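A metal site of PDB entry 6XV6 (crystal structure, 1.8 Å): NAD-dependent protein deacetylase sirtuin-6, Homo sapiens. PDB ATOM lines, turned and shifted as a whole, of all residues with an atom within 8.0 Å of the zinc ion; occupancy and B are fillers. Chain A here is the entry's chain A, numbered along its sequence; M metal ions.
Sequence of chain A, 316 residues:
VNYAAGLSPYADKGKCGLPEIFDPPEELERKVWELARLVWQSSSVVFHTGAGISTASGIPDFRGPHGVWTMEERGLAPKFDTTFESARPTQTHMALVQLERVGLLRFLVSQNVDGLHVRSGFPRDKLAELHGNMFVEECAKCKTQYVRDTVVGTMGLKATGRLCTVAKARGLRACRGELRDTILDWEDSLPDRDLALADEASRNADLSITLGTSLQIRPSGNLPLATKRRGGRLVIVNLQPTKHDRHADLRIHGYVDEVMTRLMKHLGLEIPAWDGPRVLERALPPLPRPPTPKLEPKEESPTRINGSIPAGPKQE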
ATOM      1  N   GLU A 138     -12.700 -16.767  -4.857  1.00  0.00           N
ATOM      2  CA  GLU A 138     -13.028 -16.580  -3.434  1.00  0.00           C
ATOM      3  C   GLU A 138     -13.894 -17.744  -2.958  1.00  0.00           C
ATOM      4  O   GLU A 138     -14.812 -18.149  -3.691  1.00  0.00           O
ATOM      5  CB  GLU A 138     -13.745 -15.244  -3.257  1.00  0.00           C
ATOM      6  CG  GLU A 138     -14.092 -14.948  -1.812  1.00  0.00           C
ATOM      7  CD  GLU A 138     -14.732 -13.594  -1.602  1.00  0.00           C
ATOM      8  OE1 GLU A 138     -14.108 -12.593  -2.021  1.00  0.00           O
ATOM      9  OE2 GLU A 138     -15.834 -13.550  -1.006  1.00  0.00           O
ATOM     10  N   CYS A 139     -13.595 -18.266  -1.771  1.00  0.00           N
ATOM     11  CA  CYS A 139     -14.366 -19.356  -1.122  1.00  0.00           C
ATOM     12  C   CYS A 139     -15.721 -18.797  -0.653  1.00  0.00           C
ATOM     13  O   CYS A 139     -15.715 -17.844   0.154  1.00  0.00           O
ATOM     14  CB  CYS A 139     -13.616 -19.933   0.067  1.00  0.00           C
ATOM     15  SG  CYS A 139     -14.513 -21.333   0.790  1.00  0.00           S
ATOM     16  N   ALA A 140     -16.817 -19.372  -1.147  1.00  0.00           N
ATOM     17  CA  ALA A 140     -18.198 -19.014  -0.748  1.00  0.00           C
ATOM     18  C   ALA A 140     -18.392 -19.217   0.763  1.00  0.00           C
ATOM     19  O   ALA A 140     -19.160 -18.432   1.330  1.00  0.00           O
ATOM     20  CB  ALA A 140     -19.190 -19.808  -1.557  1.00  0.00           C
ATOM     21  N   LYS A 141     -17.702 -20.175   1.395  1.00  0.00           N
ATOM     22  CA  LYS A 141     -17.857 -20.512   2.841  1.00  0.00           C
ATOM     23  C   LYS A 141     -16.999 -19.577   3.724  1.00  0.00           C
ATOM     24  O   LYS A 141     -17.600 -18.907   4.583  1.00  0.00           O
ATOM     25  CB  LYS A 141     -17.559 -21.986   3.129  1.00  0.00           C
ATOM     26  CG  LYS A 141     -18.363 -23.011   2.344  1.00  0.00           C
ATOM     27  CD  LYS A 141     -18.782 -24.273   3.111  1.00  0.00           C
ATOM     28  CE  LYS A 141     -17.698 -25.083   3.781  1.00  0.00           C
ATOM     29  NZ  LYS A 141     -17.217 -24.470   5.042  1.00  0.00           N
ATOM     30  N   CYS A 142     -15.666 -19.536   3.568  1.00  0.00           N
ATOM     31  CA  CYS A 142     -14.754 -18.846   4.527  1.00  0.00           C
ATOM     32  C   CYS A 142     -14.274 -17.478   3.992  1.00  0.00           C
ATOM     33  O   CYS A 142     -13.634 -16.739   4.767  1.00  0.00           O
ATOM     34  CB  CYS A 142     -13.560 -19.719   4.911  1.00  0.00           C
ATOM     35  SG  CYS A 142     -12.492 -20.301   3.552  1.00  0.00           S
ATOM     36  N   LYS A 143     -14.551 -17.145   2.712  1.00  0.00           N
ATOM     37  CA  LYS A 143     -14.211 -15.841   2.074  1.00  0.00           C
ATOM     38  C   LYS A 143     -12.699 -15.745   1.779  1.00  0.00           C
ATOM     39  O   LYS A 143     -12.273 -14.649   1.351  1.00  0.00           O
ATOM     40  CB  LYS A 143     -14.615 -14.639   2.935  1.00  0.00           C
ATOM     41  CG  LYS A 143     -16.075 -14.579   3.343  1.00  0.00           C
ATOM     42  CD  LYS A 143     -17.057 -14.946   2.244  1.00  0.00           C
ATOM     43  CE  LYS A 143     -18.492 -14.663   2.645  1.00  0.00           C
ATOM     44  NZ  LYS A 143     -19.445 -15.416   1.786  1.00  0.00           N
ATOM     45  N   THR A 144     -11.916 -16.801   1.990  1.00  0.00           N
ATOM     46  CA  THR A 144     -10.480 -16.816   1.611  1.00  0.00           C
ATOM     47  C   THR A 144     -10.372 -16.592   0.095  1.00  0.00           C
ATOM     48  O   THR A 144     -11.110 -17.231  -0.664  1.00  0.00           O
ATOM     49  CB  THR A 144      -9.782 -18.130   2.001  1.00  0.00           C
ATOM     50  OG1 THR A 144      -9.887 -18.259   3.419  1.00  0.00           O
ATOM     51  CG2 THR A 144      -8.307 -18.156   1.629  1.00  0.00           C
ATOM     52  N   GLN A 145      -9.472 -15.709  -0.318  1.00  0.00           N
ATOM     53  CA  GLN A 145      -9.213 -15.408  -1.747  1.00  0.00           C
ATOM     54  C   GLN A 145      -7.942 -16.122  -2.206  1.00  0.00           C
ATOM     55  O   GLN A 145      -7.042 -16.319  -1.396  1.00  0.00           O
ATOM     56  CB  GLN A 145      -9.145 -13.897  -1.938  1.00  0.00           C
ATOM     57  CG  GLN A 145     -10.507 -13.255  -1.745  1.00  0.00           C
ATOM     58  CD  GLN A 145     -10.518 -11.802  -2.133  1.00  0.00           C
ATOM     59  OE1 GLN A 145      -9.507 -11.133  -2.025  1.00  0.00           O
ATOM     60  NE2 GLN A 145     -11.666 -11.329  -2.568  1.00  0.00           N
ATOM     61  N   TYR A 146      -7.929 -16.552  -3.452  1.00  0.00           N
ATOM     62  CA  TYR A 146      -6.767 -17.199  -4.107  1.00  0.00           C
ATOM     63  C   TYR A 146      -6.411 -16.351  -5.318  1.00  0.00           C
ATOM     64  O   TYR A 146      -7.287 -16.147  -6.200  1.00  0.00           O
ATOM     65  CB  TYR A 146      -7.091 -18.624  -4.531  1.00  0.00           C
ATOM     66  CG  TYR A 146      -7.459 -19.517  -3.369  1.00  0.00           C
ATOM     67  CD1 TYR A 146      -8.694 -19.402  -2.741  1.00  0.00           C
ATOM     68  CD2 TYR A 146      -6.537 -20.426  -2.857  1.00  0.00           C
ATOM     69  CE1 TYR A 146      -9.020 -20.211  -1.657  1.00  0.00           C
ATOM     70  CE2 TYR A 146      -6.858 -21.255  -1.788  1.00  0.00           C
ATOM     71  CZ  TYR A 146      -8.096 -21.131  -1.174  1.00  0.00           C
ATOM     72  OH  TYR A 146      -8.398 -21.945  -0.098  1.00  0.00           O
ATOM     73  N   LEU A 163     -12.070 -26.237  -5.222  1.00  0.00           N
ATOM     74  CA  LEU A 163     -12.551 -26.201  -3.823  1.00  0.00           C
ATOM     75  C   LEU A 163     -11.494 -25.547  -2.946  1.00  0.00           C
ATOM     76  O   LEU A 163     -10.302 -25.601  -3.282  1.00  0.00           O
ATOM     77  CB  LEU A 163     -12.880 -27.625  -3.355  1.00  0.00           C
ATOM     78  CG  LEU A 163     -13.965 -28.338  -4.175  1.00  0.00           C
ATOM     79  CD1 LEU A 163     -14.121 -29.790  -3.748  1.00  0.00           C
ATOM     80  CD2 LEU A 163     -15.301 -27.606  -4.075  1.00  0.00           C
ATOM     81  N   CYS A 164     -11.935 -24.963  -1.837  1.00  0.00           N
ATOM     82  CA  CYS A 164     -11.079 -24.276  -0.848  1.00  0.00           C
ATOM     83  C   CYS A 164     -10.161 -25.302  -0.188  1.00  0.00           C
ATOM     84  O   CYS A 164     -10.637 -26.420   0.065  1.00  0.00           O
ATOM     85  CB  CYS A 164     -11.928 -23.587   0.187  1.00  0.00           C
ATOM     86  SG  CYS A 164     -10.960 -22.543   1.294  1.00  0.00           S
ATOM     87  N   THR A 165      -8.931 -24.909   0.126  1.00  0.00           N
ATOM     88  CA  THR A 165      -7.875 -25.797   0.669  1.00  0.00           C
ATOM     89  C   THR A 165      -7.433 -25.307   2.058  1.00  0.00           C
ATOM     90  O   THR A 165      -6.435 -25.848   2.519  1.00  0.00           O
ATOM     91  CB  THR A 165      -6.669 -25.885  -0.283  1.00  0.00           C
ATOM     92  OG1 THR A 165      -6.181 -24.548  -0.500  1.00  0.00           O
ATOM     93  CG2 THR A 165      -7.016 -26.547  -1.611  1.00  0.00           C
ATOM     94  N   VAL A 166      -8.141 -24.374   2.687  1.00  0.00           N
ATOM     95  CA  VAL A 166      -7.759 -23.827   4.021  1.00  0.00           C
ATOM     96  C   VAL A 166      -8.025 -24.909   5.067  1.00  0.00           C
ATOM     97  O   VAL A 166      -9.069 -25.557   5.003  1.00  0.00           O
ATOM     98  CB  VAL A 166      -8.494 -22.517   4.382  1.00  0.00           C
ATOM     99  CG1 VAL A 166      -8.377 -22.149   5.857  1.00  0.00           C
ATOM    100  CG2 VAL A 166      -8.039 -21.348   3.514  1.00  0.00           C
ATOM    101  N   ALA A 167      -7.082 -25.086   6.003  1.00  0.00           N
ATOM    102  CA  ALA A 167      -7.256 -25.839   7.266  1.00  0.00           C
ATOM    103  C   ALA A 167      -7.821 -24.905   8.344  1.00  0.00           C
ATOM    104  O   ALA A 167      -8.800 -25.325   8.985  1.00  0.00           O
ATOM    105  CB  ALA A 167      -5.931 -26.412   7.704  1.00  0.00           C
ATOM    106  N   CYS A 175     -11.579 -26.953   4.561  1.00  0.00           N
ATOM    107  CA  CYS A 175     -12.811 -26.142   4.347  1.00  0.00           C
ATOM    108  C   CYS A 175     -13.666 -26.755   3.238  1.00  0.00           C
ATOM    109  O   CYS A 175     -14.866 -26.980   3.448  1.00  0.00           O
ATOM    110  CB  CYS A 175     -12.484 -24.699   3.993  1.00  0.00           C
ATOM    111  SG  CYS A 175     -13.935 -23.734   3.531  1.00  0.00           S
ATOM    112  N   ARG A 176     -13.077 -26.972   2.062  1.00  0.00           N
ATOM    113  CA  ARG A 176     -13.718 -27.574   0.876  1.00  0.00           C
ATOM    114  C   ARG A 176     -14.868 -26.689   0.357  1.00  0.00           C
ATOM    115  O   ARG A 176     -15.586 -27.157  -0.551  1.00  0.00           O
ATOM    116  CB  ARG A 176     -14.180 -29.008   1.178  1.00  0.00           C
ATOM    117  CG  ARG A 176     -13.079 -29.976   1.578  1.00  0.00           C
ATOM    118  CD  ARG A 176     -13.647 -31.324   1.996  1.00  0.00           C
ATOM    119  NE  ARG A 176     -14.507 -31.939   0.979  1.00  0.00           N
ATOM    120  CZ  ARG A 176     -15.838 -32.113   1.065  1.00  0.00           C
ATOM    121  NH1 ARG A 176     -16.513 -31.710   2.137  1.00  0.00           N
ATOM    122  NH2 ARG A 176     -16.496 -32.689   0.063  1.00  0.00           N
ATOM    123  N   GLY A 177     -15.007 -25.450   0.821  1.00  0.00           N
ATOM    124  CA  GLY A 177     -15.955 -24.474   0.247  1.00  0.00           C
ATOM    125  C   GLY A 177     -15.798 -24.331  -1.271  1.00  0.00           C
ATOM    126  O   GLY A 177     -14.701 -24.613  -1.818  1.00  0.00           O
ATOM    127  N   GLU A 178     -16.878 -23.953  -1.956  1.00  0.00           N
ATOM    128  CA  GLU A 178     -16.917 -23.745  -3.419  1.00  0.00           C
ATOM    129  C   GLU A 178     -16.176 -22.438  -3.728  1.00  0.00           C
ATOM    130  O   GLU A 178     -16.529 -21.386  -3.159  1.00  0.00           O
ATOM    131  CB  GLU A 178     -18.366 -23.686  -3.924  1.00  0.00           C
ATOM    132  N   LEU A 179     -15.160 -22.491  -4.597  1.00  0.00           N
ATOM    133  CA  LEU A 179     -14.459 -21.275  -5.061  1.00  0.00           C
ATOM    134  C   LEU A 179     -15.298 -20.649  -6.169  1.00  0.00           C
ATOM    135  O   LEU A 179     -15.781 -21.389  -7.048  1.00  0.00           O
ATOM    136  CB  LEU A 179     -13.034 -21.611  -5.525  1.00  0.00           C
ATOM    137  CG  LEU A 179     -12.107 -22.215  -4.468  1.00  0.00           C
ATOM    138  CD1 LEU A 179     -10.665 -22.177  -4.967  1.00  0.00           C
ATOM    139  CD2 LEU A 179     -12.246 -21.529  -3.127  1.00  0.00           C
HETATM  140 ZN    ZN M   1     -12.928 -21.851   2.402  1.00  0.00          ZN
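SG of Cys 175 lies close to N of Gly 177. N of Cys 139 lies within hydrogen-bond range of O of Thr 144. O of Cys 164 lies within hydrogen-bond range of N of Arg 176 (3.2 Å). The side-chain sulfur (SG) of Cys 139 sits close to the backbone NH (N) of Lys 141 (3.4 Å). OH of Tyr 146 lies close to SG of Cys 164, at 3.0 Å. The side-chain sulfur of Cys 175 lies close to the side-chain amino group of Lys 141, at 3.7 Å. SG of Cys 164 lies close to N of Val 166, 3.6 Å away. The backbone NH of Cys 164 sits at hydrogen-bond distance from the backbone carbonyl oxygen of Gly 177.
Along chain A the residues within 4 Å of the zinc ion span positions 139 to 175. The nearest printed residue that does not touch the zinc ion is Gly 177 (4.4 Å).
The side-chain sulfur (SG) of Cys 142 binds the zinc ion, at 2.0 Å. The zinc ion is bound by SG of Cys 139. The zinc ion is bound by SG of Cys 164, at 2.4 Å. SG of Cys 175 is bound to the zinc ion, at 2.4 Å. The zinc ion has four donor atoms within binding distance.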
